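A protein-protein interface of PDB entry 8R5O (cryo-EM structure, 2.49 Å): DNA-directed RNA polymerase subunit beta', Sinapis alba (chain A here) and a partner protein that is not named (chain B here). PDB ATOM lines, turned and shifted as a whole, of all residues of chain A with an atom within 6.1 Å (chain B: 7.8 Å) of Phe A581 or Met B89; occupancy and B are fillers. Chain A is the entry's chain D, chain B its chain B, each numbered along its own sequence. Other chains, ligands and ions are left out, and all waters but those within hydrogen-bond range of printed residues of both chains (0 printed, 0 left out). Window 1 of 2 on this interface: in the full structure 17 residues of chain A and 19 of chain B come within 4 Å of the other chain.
The side-chain carboxylate (OE1) of Glu B86 is in salt-bridge range of the guanidinium group (NH2) of Arg A605, 3.4 Å away. The side-chain carboxylate (OE1) of Glu B86 is in hydrogen-bond range of the side-chain hydroxyl (OH) of Tyr A651. The side-chain amide oxygen of Asn B90 is in hydrogen-bond range of the guanidinium group of Arg A605 (3.2 Å). The side-chain carboxylate (OE2) of Glu B93 lies within hydrogen-bond range of the side-chain amide nitrogen (ND2) of Asn A583, 3.3 Å away. The side-chain carboxylate (OE1) of Glu B93 is in salt-bridge range of the guanidinium group (NH1) of Arg A605. The backbone carbonyl oxygen (O) of Phe A580 sits close to the side-chain carboxylate (OD2) of Asp B173, at 3.3 Å.
A ring nitrogen (NE2) of His B85 sits at hydrogen-bond distance from the side-chain sulfur (SD) of Met B89. The backbone carbonyl oxygen (O) of Glu B86 sits close to the side-chain amide nitrogen (ND2) of Asn B90 (3.4 Å). O of Ile B136 lies within hydrogen-bond range of ND2 of Asn B90 (2.9 Å). O of Phe A581 lies within hydrogen-bond range of N of Arg A605 (3.1 Å). The side-chain carboxylate (OD2) of Asp A586 lies within hydrogen-bond range of the side-chain sulfur (SG) of Cys A582 (3.2 Å). The side-chain amide oxygen (OD1) of Asn A583 sits at hydrogen-bond distance from the backbone NH (N) of Asp A586 (3.0 Å).
Among the printed residues, merely in contact across the chains: Phe A580 with His B85, Phe A581 with Met B89, Cys A582 with Glu B93, Asp A586 with Met B177, Arg A605 with Met B89 and Tyr A651 with His B85.
Phe A581 touches just one residue of chain B: Met B89 (3.9 Å). Of the printed residues of chain B, Asp A586 touches Met B177. Val B84 touches none of the printed residues of chain A. Of the printed residues of chain A, His B85 touches Phe A580 (3.5 Å) and Tyr A651 (3.7 Å). Of chain A, only Phe A581 (3.9 Å) and Arg A605 (3.7 Å) come within 4 Å of Met B89. Printed residues of chain A within 4 Å of Asn B90: Arg A605 (3.2 Å). Printed residues of chain A within 4 Å of Met B177: Asp A586. The nearest residue of chain A that does not touch Met B89 is Cys A582 (4.1 Å). The nearest printed residue of chain A that does not touch Asp B173 is Pro A579 (4.2 Å).
Of the 17 printed residues of chain A, 7 touch a printed residue of chain B. Hydrophobic or aromatic side chains of chain A that line the printed part of chain B: Phe A580 and Tyr A651. Hydrophobic or aromatic side chains of chain B that line the printed part of chain A: His B85, Met B89 and Met B177. Among the printed residues, Asp or Glu carboxylates within 4 Å of a Lys or Arg side-chain nitrogen of the other chain: Arg A605 with Glu B86 (3.4 Å) and Arg A605 with Glu B93 (3.98 Å).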
ATOM      1  N   PRO A 579       7.609 -13.933  -2.481  1.00  0.00           N
ATOM      2  CA  PRO A 579       7.909 -15.055  -1.586  1.00  0.00           C
ATOM      3  C   PRO A 579       9.383 -15.136  -1.214  1.00  0.00           C
ATOM      4  O   PRO A 579      10.270 -14.785  -1.993  1.00  0.00           O
ATOM      5  CB  PRO A 579       7.478 -16.279  -2.399  1.00  0.00           C
ATOM      6  CG  PRO A 579       7.557 -15.834  -3.814  1.00  0.00           C
ATOM      7  CD  PRO A 579       7.173 -14.389  -3.811  1.00  0.00           C
ATOM      8  N   PHE A 580       9.627 -15.613   0.002  1.00  0.00           N
ATOM      9  CA  PHE A 580      10.962 -15.927   0.493  1.00  0.00           C
ATOM     10  C   PHE A 580      11.119 -17.439   0.550  1.00  0.00           C
ATOM     11  O   PHE A 580      10.226 -18.138   1.037  1.00  0.00           O
ATOM     12  CB  PHE A 580      11.203 -15.324   1.877  1.00  0.00           C
ATOM     13  CG  PHE A 580      11.755 -13.930   1.850  1.00  0.00           C
ATOM     14  CD1 PHE A 580      10.931 -12.848   1.595  1.00  0.00           C
ATOM     15  CD2 PHE A 580      13.097 -13.701   2.097  1.00  0.00           C
ATOM     16  CE1 PHE A 580      11.439 -11.565   1.577  1.00  0.00           C
ATOM     17  CE2 PHE A 580      13.611 -12.420   2.081  1.00  0.00           C
ATOM     18  CZ  PHE A 580      12.781 -11.351   1.819  1.00  0.00           C
ATOM     19  N   PHE A 581      12.246 -17.939   0.057  1.00  0.00           N
ATOM     20  CA  PHE A 581      12.535 -19.365   0.063  1.00  0.00           C
ATOM     21  C   PHE A 581      13.812 -19.617   0.848  1.00  0.00           C
ATOM     22  O   PHE A 581      14.808 -18.910   0.668  1.00  0.00           O
ATOM     23  CB  PHE A 581      12.654 -19.911  -1.361  1.00  0.00           C
ATOM     24  CG  PHE A 581      11.361 -19.893  -2.120  1.00  0.00           C
ATOM     25  CD1 PHE A 581      10.382 -20.836  -1.861  1.00  0.00           C
ATOM     26  CD2 PHE A 581      11.122 -18.934  -3.087  1.00  0.00           C
ATOM     27  CE1 PHE A 581       9.190 -20.823  -2.553  1.00  0.00           C
ATOM     28  CE2 PHE A 581       9.932 -18.917  -3.783  1.00  0.00           C
ATOM     29  CZ  PHE A 581       8.964 -19.863  -3.516  1.00  0.00           C
ATOM     30  N   CYS A 582      13.773 -20.625   1.722  1.00  0.00           N
ATOM     31  CA  CYS A 582      14.923 -20.927   2.567  1.00  0.00           C
ATOM     32  C   CYS A 582      16.090 -21.468   1.750  1.00  0.00           C
ATOM     33  O   CYS A 582      17.252 -21.173   2.049  1.00  0.00           O
ATOM     34  CB  CYS A 582      14.522 -21.916   3.659  1.00  0.00           C
ATOM     35  SG  CYS A 582      13.673 -23.393   3.053  1.00  0.00           S
ATOM     36  N   ASN A 583      15.805 -22.263   0.721  1.00  0.00           N
ATOM     37  CA  ASN A 583      16.847 -22.815  -0.132  1.00  0.00           C
ATOM     38  C   ASN A 583      16.314 -22.934  -1.551  1.00  0.00           C
ATOM     39  O   ASN A 583      15.121 -22.752  -1.809  1.00  0.00           O
ATOM     40  CB  ASN A 583      17.342 -24.169   0.389  1.00  0.00           C
ATOM     41  CG  ASN A 583      16.209 -25.102   0.764  1.00  0.00           C
ATOM     42  OD1 ASN A 583      15.580 -25.711  -0.097  1.00  0.00           O
ATOM     43  ND2 ASN A 583      15.951 -25.222   2.059  1.00  0.00           N
ATOM     44  N   SER A 584      17.220 -23.246  -2.478  1.00  0.00           N
ATOM     45  CA  SER A 584      16.851 -23.294  -3.889  1.00  0.00           C
ATOM     46  C   SER A 584      15.936 -24.471  -4.198  1.00  0.00           C
ATOM     47  O   SER A 584      15.142 -24.401  -5.142  1.00  0.00           O
ATOM     48  CB  SER A 584      18.106 -23.360  -4.756  1.00  0.00           C
ATOM     49  OG  SER A 584      18.772 -24.597  -4.586  1.00  0.00           O
ATOM     50  N   ASP A 586      13.475 -25.627  -2.277  1.00  0.00           N
ATOM     51  CA  ASP A 586      12.105 -25.221  -1.976  1.00  0.00           C
ATOM     52  C   ASP A 586      11.532 -24.344  -3.082  1.00  0.00           C
ATOM     53  O   ASP A 586      10.354 -24.471  -3.432  1.00  0.00           O
ATOM     54  CB  ASP A 586      12.043 -24.496  -0.632  1.00  0.00           C
ATOM     55  CG  ASP A 586      11.999 -25.449   0.544  1.00  0.00           C
ATOM     56  OD1 ASP A 586      12.508 -26.581   0.419  1.00  0.00           O
ATOM     57  OD2 ASP A 586      11.439 -25.071   1.595  1.00  0.00           O
ATOM     58  N   ALA A 587      12.348 -23.443  -3.635  1.00  0.00           N
ATOM     59  CA  ALA A 587      11.876 -22.590  -4.721  1.00  0.00           C
ATOM     60  C   ALA A 587      11.533 -23.410  -5.957  1.00  0.00           C
ATOM     61  O   ALA A 587      10.509 -23.171  -6.607  1.00  0.00           O
ATOM     62  CB  ALA A 587      12.927 -21.533  -5.055  1.00  0.00           C
ATOM     63  N   ILE A 588      12.378 -24.383  -6.296  1.00  0.00           N
ATOM     64  CA  ILE A 588      12.099 -25.239  -7.442  1.00  0.00           C
ATOM     65  C   ILE A 588      10.885 -26.117  -7.169  1.00  0.00           C
ATOM     66  O   ILE A 588      10.068 -26.365  -8.063  1.00  0.00           O
ATOM     67  CB  ILE A 588      13.345 -26.070  -7.797  1.00  0.00           C
ATOM     68  CG1 ILE A 588      14.473 -25.146  -8.260  1.00  0.00           C
ATOM     69  CG2 ILE A 588      13.021 -27.099  -8.868  1.00  0.00           C
ATOM     70  CD1 ILE A 588      15.742 -25.865  -8.633  1.00  0.00           C
ATOM     71  N   ALA A 590       8.304 -25.348  -5.260  1.00  0.00           N
ATOM     72  CA  ALA A 590       7.125 -24.503  -5.406  1.00  0.00           C
ATOM     73  C   ALA A 590       6.791 -24.257  -6.871  1.00  0.00           C
ATOM     74  O   ALA A 590       5.615 -24.109  -7.222  1.00  0.00           O
ATOM     75  CB  ALA A 590       7.335 -23.176  -4.679  1.00  0.00           C
ATOM     76  N   ILE A 596       4.520 -20.738  -8.253  1.00  0.00           N
ATOM     77  CA  ILE A 596       5.163 -19.576  -8.844  1.00  0.00           C
ATOM     78  C   ILE A 596       5.422 -19.870 -10.314  1.00  0.00           C
ATOM     79  O   ILE A 596       5.427 -21.022 -10.752  1.00  0.00           O
ATOM     80  CB  ILE A 596       6.481 -19.197  -8.134  1.00  0.00           C
ATOM     81  CG1 ILE A 596       7.454 -20.376  -8.153  1.00  0.00           C
ATOM     82  CG2 ILE A 596       6.217 -18.739  -6.709  1.00  0.00           C
ATOM     83  CD1 ILE A 596       8.750 -20.098  -7.444  1.00  0.00           C
ATOM     84  N   LEU A 602      11.521 -13.643  -6.800  1.00  0.00           N
ATOM     85  CA  LEU A 602      11.521 -14.242  -5.474  1.00  0.00           C
ATOM     86  C   LEU A 602      12.813 -13.872  -4.766  1.00  0.00           C
ATOM     87  O   LEU A 602      13.790 -13.456  -5.390  1.00  0.00           O
ATOM     88  CB  LEU A 602      11.356 -15.768  -5.539  1.00  0.00           C
ATOM     89  CG  LEU A 602      12.379 -16.595  -6.331  1.00  0.00           C
ATOM     90  CD1 LEU A 602      13.585 -16.987  -5.485  1.00  0.00           C
ATOM     91  CD2 LEU A 602      11.722 -17.831  -6.920  1.00  0.00           C
ATOM     92  N   TRP A 603      12.807 -14.037  -3.448  1.00  0.00           N
ATOM     93  CA  TRP A 603      13.997 -13.851  -2.633  1.00  0.00           C
ATOM     94  C   TRP A 603      14.532 -15.212  -2.219  1.00  0.00           C
ATOM     95  O   TRP A 603      13.771 -16.070  -1.763  1.00  0.00           O
ATOM     96  CB  TRP A 603      13.693 -13.001  -1.400  1.00  0.00           C
ATOM     97  CG  TRP A 603      13.377 -11.582  -1.723  1.00  0.00           C
ATOM     98  CD1 TRP A 603      12.141 -11.029  -1.861  1.00  0.00           C
ATOM     99  CD2 TRP A 603      14.317 -10.529  -1.959  1.00  0.00           C
ATOM    100  NE1 TRP A 603      12.251  -9.694  -2.163  1.00  0.00           N
ATOM    101  CE2 TRP A 603      13.578  -9.363  -2.229  1.00  0.00           C
ATOM    102  CE3 TRP A 603      15.712 -10.460  -1.967  1.00  0.00           C
ATOM    103  CZ2 TRP A 603      14.186  -8.142  -2.503  1.00  0.00           C
ATOM    104  CZ3 TRP A 603      16.313  -9.250  -2.238  1.00  0.00           C
ATOM    105  CH2 TRP A 603      15.552  -8.106  -2.502  1.00  0.00           C
ATOM    106  N   LEU A 604      15.833 -15.410  -2.388  1.00  0.00           N
ATOM    107  CA  LEU A 604      16.484 -16.673  -2.068  1.00  0.00           C
ATOM    108  C   LEU A 604      17.470 -16.448  -0.933  1.00  0.00           C
ATOM    109  O   LEU A 604      18.379 -15.622  -1.051  1.00  0.00           O
ATOM    110  CB  LEU A 604      17.197 -17.248  -3.292  1.00  0.00           C
ATOM    111  CG  LEU A 604      18.069 -18.481  -3.054  1.00  0.00           C
ATOM    112  CD1 LEU A 604      17.229 -19.655  -2.580  1.00  0.00           C
ATOM    113  CD2 LEU A 604      18.843 -18.843  -4.309  1.00  0.00           C
ATOM    114  N   ARG A 605      17.284 -17.179   0.162  1.00  0.00           N
ATOM    115  CA  ARG A 605      18.268 -17.184   1.234  1.00  0.00           C
ATOM    116  C   ARG A 605      19.581 -17.757   0.718  1.00  0.00           C
ATOM    117  O   ARG A 605      19.622 -18.870   0.192  1.00  0.00           O
ATOM    118  CB  ARG A 605      17.747 -18.005   2.413  1.00  0.00           C
ATOM    119  CG  ARG A 605      18.543 -17.875   3.696  1.00  0.00           C
ATOM    120  CD  ARG A 605      18.031 -18.861   4.736  1.00  0.00           C
ATOM    121  NE  ARG A 605      18.572 -18.605   6.065  1.00  0.00           N
ATOM    122  CZ  ARG A 605      18.324 -19.353   7.131  1.00  0.00           C
ATOM    123  NH1 ARG A 605      17.552 -20.424   7.059  1.00  0.00           N
ATOM    124  NH2 ARG A 605      18.865 -19.019   8.299  1.00  0.00           N
ATOM    125  N   TYR A 651      20.281 -12.191   0.888  1.00  0.00           N
ATOM    126  CA  TYR A 651      19.097 -12.651   0.176  1.00  0.00           C
ATOM    127  C   TYR A 651      19.162 -12.126  -1.246  1.00  0.00           C
ATOM    128  O   TYR A 651      19.316 -10.920  -1.457  1.00  0.00           O
ATOM    129  CB  TYR A 651      17.810 -12.182   0.860  1.00  0.00           C
ATOM    130  CG  TYR A 651      17.741 -12.535   2.324  1.00  0.00           C
ATOM    131  CD1 TYR A 651      18.207 -11.656   3.288  1.00  0.00           C
ATOM    132  CD2 TYR A 651      17.214 -13.747   2.743  1.00  0.00           C
ATOM    133  CE1 TYR A 651      18.149 -11.969   4.626  1.00  0.00           C
ATOM    134  CE2 TYR A 651      17.152 -14.070   4.084  1.00  0.00           C
ATOM    135  CZ  TYR A 651      17.622 -13.176   5.020  1.00  0.00           C
ATOM    136  OH  TYR A 651      17.568 -13.484   6.359  1.00  0.00           O
ATOM    137  N   VAL A 656      13.289 -18.626 -10.517  1.00  0.00           N
ATOM    138  CA  VAL A 656      13.620 -20.043 -10.600  1.00  0.00           C
ATOM    139  C   VAL A 656      14.358 -20.371 -11.887  1.00  0.00           C
ATOM    140  O   VAL A 656      15.087 -21.365 -11.938  1.00  0.00           O
ATOM    141  CB  VAL A 656      12.366 -20.926 -10.465  1.00  0.00           C
ATOM    142  CG1 VAL A 656      11.906 -20.968  -9.022  1.00  0.00           C
ATOM    143  CG2 VAL A 656      11.263 -20.421 -11.364  1.00  0.00           C
ATOM    144  N   SER B  83      17.788 -12.700  14.158  1.00  0.00           N
ATOM    145  CA  SER B  83      16.645 -11.813  14.037  1.00  0.00           C
ATOM    146  C   SER B  83      15.349 -12.621  13.974  1.00  0.00           C
ATOM    147  O   SER B  83      15.348 -13.854  13.914  1.00  0.00           O
ATOM    148  CB  SER B  83      16.785 -10.931  12.798  1.00  0.00           C
ATOM    149  OG  SER B  83      17.081 -11.706  11.651  1.00  0.00           O
ATOM    150  N   VAL B  84      14.226 -11.900  13.993  1.00  0.00           N
ATOM    151  CA  VAL B  84      12.921 -12.552  13.933  1.00  0.00           C
ATOM    152  C   VAL B  84      12.754 -13.293  12.613  1.00  0.00           C
ATOM    153  O   VAL B  84      12.246 -14.421  12.577  1.00  0.00           O
ATOM    154  CB  VAL B  84      11.800 -11.519  14.153  1.00  0.00           C
ATOM    155  CG1 VAL B  84      10.436 -12.152  13.933  1.00  0.00           C
ATOM    156  CG2 VAL B  84      11.897 -10.931  15.550  1.00  0.00           C
ATOM    157  N   HIS B  85      13.181 -12.676  11.509  1.00  0.00           N
ATOM    158  CA  HIS B  85      13.029 -13.307  10.202  1.00  0.00           C
ATOM    159  C   HIS B  85      13.856 -14.583  10.101  1.00  0.00           C
ATOM    160  O   HIS B  85      13.400 -15.577   9.529  1.00  0.00           O
ATOM    161  CB  HIS B  85      13.412 -12.323   9.098  1.00  0.00           C
ATOM    162  CG  HIS B  85      13.101 -12.813   7.717  1.00  0.00           C
ATOM    163  ND1 HIS B  85      11.817 -13.092   7.300  1.00  0.00           N
ATOM    164  CD2 HIS B  85      13.905 -13.073   6.661  1.00  0.00           C
ATOM    165  CE1 HIS B  85      11.844 -13.502   6.045  1.00  0.00           C
ATOM    166  NE2 HIS B  85      13.099 -13.500   5.634  1.00  0.00           N
ATOM    167  N   GLU B  86      15.072 -14.576  10.654  1.00  0.00           N
ATOM    168  CA  GLU B  86      15.914 -15.769  10.612  1.00  0.00           C
ATOM    169  C   GLU B  86      15.293 -16.918  11.397  1.00  0.00           C
ATOM    170  O   GLU B  86      15.400 -18.081  10.993  1.00  0.00           O
ATOM    171  CB  GLU B  86      17.311 -15.448  11.143  1.00  0.00           C
ATOM    172  CG  GLU B  86      18.149 -14.568  10.229  1.00  0.00           C
ATOM    173  CD  GLU B  86      18.715 -15.316   9.036  1.00  0.00           C
ATOM    174  OE1 GLU B  86      17.933 -15.727   8.153  1.00  0.00           O
ATOM    175  OE2 GLU B  86      19.950 -15.497   8.980  1.00  0.00           O
ATOM    176  N   ILE B  87      14.651 -16.615  12.527  1.00  0.00           N
ATOM    177  CA  ILE B  87      13.943 -17.647  13.278  1.00  0.00           C
ATOM    178  C   ILE B  87      12.807 -18.225  12.444  1.00  0.00           C
ATOM    179  O   ILE B  87      12.594 -19.442  12.417  1.00  0.00           O
ATOM    180  CB  ILE B  87      13.437 -17.082  14.618  1.00  0.00           C
ATOM    181  CG1 ILE B  87      14.618 -16.656  15.488  1.00  0.00           C
ATOM    182  CG2 ILE B  87      12.593 -18.106  15.350  1.00  0.00           C
ATOM    183  CD1 ILE B  87      14.208 -16.095  16.824  1.00  0.00           C
ATOM    184  N   LEU B  88      12.063 -17.363  11.746  1.00  0.00           N
ATOM    185  CA  LEU B  88      10.994 -17.843  10.876  1.00  0.00           C
ATOM    186  C   LEU B  88      11.545 -18.708   9.749  1.00  0.00           C
ATOM    187  O   LEU B  88      10.947 -19.730   9.394  1.00  0.00           O
ATOM    188  CB  LEU B  88      10.205 -16.663  10.312  1.00  0.00           C
ATOM    189  CG  LEU B  88       9.495 -15.758  11.319  1.00  0.00           C
ATOM    190  CD1 LEU B  88       8.722 -14.671  10.597  1.00  0.00           C
ATOM    191  CD2 LEU B  88       8.576 -16.565  12.217  1.00  0.00           C
ATOM    192  N   MET B  89      12.678 -18.309   9.167  1.00  0.00           N
ATOM    193  CA  MET B  89      13.302 -19.122   8.127  1.00  0.00           C
ATOM    194  C   MET B  89      13.743 -20.474   8.675  1.00  0.00           C
ATOM    195  O   MET B  89      13.586 -21.503   8.007  1.00  0.00           O
ATOM    196  CB  MET B  89      14.491 -18.379   7.516  1.00  0.00           C
ATOM    197  CG  MET B  89      14.143 -17.030   6.912  1.00  0.00           C
ATOM    198  SD  MET B  89      13.152 -17.131   5.412  1.00  0.00           S
ATOM    199  CE  MET B  89      14.436 -17.198   4.168  1.00  0.00           C
ATOM    200  N   ASN B  90      14.308 -20.490   9.884  1.00  0.00           N
ATOM    201  CA  ASN B  90      14.712 -21.753  10.495  1.00  0.00           C
ATOM    202  C   ASN B  90      13.508 -22.636  10.798  1.00  0.00           C
ATOM    203  O   ASN B  90      13.556 -23.852  10.586  1.00  0.00           O
ATOM    204  CB  ASN B  90      15.520 -21.491  11.766  1.00  0.00           C
ATOM    205  CG  ASN B  90      16.880 -20.892  11.478  1.00  0.00           C
ATOM    206  OD1 ASN B  90      17.394 -20.997  10.365  1.00  0.00           O
ATOM    207  ND2 ASN B  90      17.475 -20.264  12.484  1.00  0.00           N
ATOM    208  N   LEU B  91      12.421 -22.044  11.299  1.00  0.00           N
ATOM    209  CA  LEU B  91      11.209 -22.816  11.554  1.00  0.00           C
ATOM    210  C   LEU B  91      10.613 -23.362  10.266  1.00  0.00           C
ATOM    211  O   LEU B  91       9.975 -24.420  10.275  1.00  0.00           O
ATOM    212  CB  LEU B  91      10.179 -21.958  12.288  1.00  0.00           C
ATOM    213  CG  LEU B  91      10.499 -21.580  13.733  1.00  0.00           C
ATOM    214  CD1 LEU B  91       9.467 -20.605  14.264  1.00  0.00           C
ATOM    215  CD2 LEU B  91      10.570 -22.822  14.606  1.00  0.00           C
ATOM    216  N   ASN B  92      10.800 -22.651   9.153  1.00  0.00           N
ATOM    217  CA  ASN B  92      10.298 -23.116   7.868  1.00  0.00           C
ATOM    218  C   ASN B  92      11.009 -24.376   7.391  1.00  0.00           C
ATOM    219  O   ASN B  92      10.449 -25.116   6.576  1.00  0.00           O
ATOM    220  CB  ASN B  92      10.440 -22.002   6.830  1.00  0.00           C
ATOM    221  CG  ASN B  92       9.555 -22.213   5.621  1.00  0.00           C
ATOM    222  OD1 ASN B  92       8.620 -23.011   5.652  1.00  0.00           O
ATOM    223  ND2 ASN B  92       9.841 -21.491   4.547  1.00  0.00           N
ATOM    224  N   GLU B  93      12.217 -24.640   7.881  1.00  0.00           N
ATOM    225  CA  GLU B  93      13.015 -25.775   7.438  1.00  0.00           C
ATOM    226  C   GLU B  93      12.831 -27.026   8.289  1.00  0.00           C
ATOM    227  O   GLU B  93      13.422 -28.061   7.968  1.00  0.00           O
ATOM    228  CB  GLU B  93      14.499 -25.396   7.413  1.00  0.00           C
ATOM    229  CG  GLU B  93      14.893 -24.484   6.269  1.00  0.00           C
ATOM    230  CD  GLU B  93      16.395 -24.320   6.152  1.00  0.00           C
ATOM    231  OE1 GLU B  93      17.081 -24.372   7.192  1.00  0.00           O
ATOM    232  OE2 GLU B  93      16.891 -24.150   5.018  1.00  0.00           O
ATOM    233  N   ILE B  94      12.034 -26.970   9.350  1.00  0.00           N
ATOM    234  CA  ILE B  94      11.880 -28.112  10.247  1.00  0.00           C
ATOM    235  C   ILE B  94      10.941 -29.128   9.612  1.00  0.00           C
ATOM    236  O   ILE B  94       9.819 -28.795   9.218  1.00  0.00           O
ATOM    237  CB  ILE B  94      11.367 -27.659  11.621  1.00  0.00           C
ATOM    238  CG1 ILE B  94      12.436 -26.831  12.332  1.00  0.00           C
ATOM    239  CG2 ILE B  94      10.967 -28.858  12.467  1.00  0.00           C
ATOM    240  CD1 ILE B  94      12.042 -26.389  13.711  1.00  0.00           C
ATOM    241  N   HIS B 135      18.337 -26.627  13.806  1.00  0.00           N
ATOM    242  CA  HIS B 135      18.570 -25.432  14.601  1.00  0.00           C
ATOM    243  C   HIS B 135      17.417 -24.443  14.463  1.00  0.00           C
ATOM    244  O   HIS B 135      16.780 -24.340  13.411  1.00  0.00           O
ATOM    245  CB  HIS B 135      19.883 -24.768  14.181  1.00  0.00           C
ATOM    246  CG  HIS B 135      20.321 -23.665  15.092  1.00  0.00           C
ATOM    247  ND1 HIS B 135      20.284 -22.337  14.725  1.00  0.00           N
ATOM    248  CD2 HIS B 135      20.803 -23.693  16.356  1.00  0.00           C
ATOM    249  CE1 HIS B 135      20.724 -21.595  15.723  1.00  0.00           C
ATOM    250  NE2 HIS B 135      21.045 -22.392  16.725  1.00  0.00           N
ATOM    251  N   ILE B 136      17.154 -23.712  15.545  1.00  0.00           N
ATOM    252  CA  ILE B 136      16.087 -22.717  15.563  1.00  0.00           C
ATOM    253  C   ILE B 136      16.649 -21.354  15.949  1.00  0.00           C
ATOM    254  O   ILE B 136      16.519 -20.381  15.198  1.00  0.00           O
ATOM    255  CB  ILE B 136      14.953 -23.129  16.519  1.00  0.00           C
ATOM    256  CG1 ILE B 136      14.278 -24.414  16.034  1.00  0.00           C
ATOM    257  CG2 ILE B 136      13.938 -22.008  16.653  1.00  0.00           C
ATOM    258  CD1 ILE B 136      13.117 -24.856  16.900  1.00  0.00           C
ATOM    259  N   ILE B 172       4.077 -18.220   7.883  1.00  0.00           N
ATOM    260  CA  ILE B 172       5.228 -18.935   7.346  1.00  0.00           C
ATOM    261  C   ILE B 172       4.793 -19.592   6.045  1.00  0.00           C
ATOM    262  O   ILE B 172       3.932 -20.481   6.050  1.00  0.00           O
ATOM    263  CB  ILE B 172       5.773 -19.972   8.339  1.00  0.00           C
ATOM    264  CG1 ILE B 172       6.333 -19.270   9.578  1.00  0.00           C
ATOM    265  CG2 ILE B 172       6.837 -20.836   7.677  1.00  0.00           C
ATOM    266  CD1 ILE B 172       6.840 -20.209  10.642  1.00  0.00           C
ATOM    267  N   ASP B 173       5.381 -19.153   4.937  1.00  0.00           N
ATOM    268  CA  ASP B 173       5.026 -19.665   3.615  1.00  0.00           C
ATOM    269  C   ASP B 173       5.678 -21.030   3.442  1.00  0.00           C
ATOM    270  O   ASP B 173       6.770 -21.162   2.890  1.00  0.00           O
ATOM    271  CB  ASP B 173       5.452 -18.687   2.527  1.00  0.00           C
ATOM    272  CG  ASP B 173       6.820 -18.083   2.784  1.00  0.00           C
ATOM    273  OD1 ASP B 173       7.491 -18.513   3.746  1.00  0.00           O
ATOM    274  OD2 ASP B 173       7.223 -17.174   2.025  1.00  0.00           O
ATOM    275  N   ALA B 174       4.994 -22.061   3.928  1.00  0.00           N
ATOM    276  CA  ALA B 174       5.509 -23.418   3.861  1.00  0.00           C
ATOM    277  C   ALA B 174       5.201 -24.047   2.510  1.00  0.00           C
ATOM    278  O   ALA B 174       4.127 -23.836   1.939  1.00  0.00           O
ATOM    279  CB  ALA B 174       4.914 -24.269   4.982  1.00  0.00           C
ATOM    280  N   VAL B 175       6.153 -24.816   1.997  1.00  0.00           N
ATOM    281  CA  VAL B 175       5.963 -25.607   0.788  1.00  0.00           C
ATOM    282  C   VAL B 175       5.781 -27.053   1.227  1.00  0.00           C
ATOM    283  O   VAL B 175       6.713 -27.678   1.743  1.00  0.00           O
ATOM    284  CB  VAL B 175       7.141 -25.454  -0.185  1.00  0.00           C
ATOM    285  CG1 VAL B 175       6.858 -26.186  -1.490  1.00  0.00           C
ATOM    286  CG2 VAL B 175       7.427 -23.984  -0.446  1.00  0.00           C
ATOM    287  N   MET B 177       5.938 -30.461   0.593  1.00  0.00           N
ATOM    288  CA  MET B 177       6.506 -31.453  -0.322  1.00  0.00           C
ATOM    289  C   MET B 177       7.373 -32.434   0.452  1.00  0.00           C
ATOM    290  O   MET B 177       8.602 -32.311   0.498  1.00  0.00           O
ATOM    291  CB  MET B 177       7.296 -30.786  -1.450  1.00  0.00           C
ATOM    292  CG  MET B 177       8.246 -29.686  -1.019  1.00  0.00           C
ATOM    293  SD  MET B 177       9.322 -29.191  -2.375  1.00  0.00           S
ATOM    294  CE  MET B 177      10.689 -28.487  -1.471  1.00  0.00           C
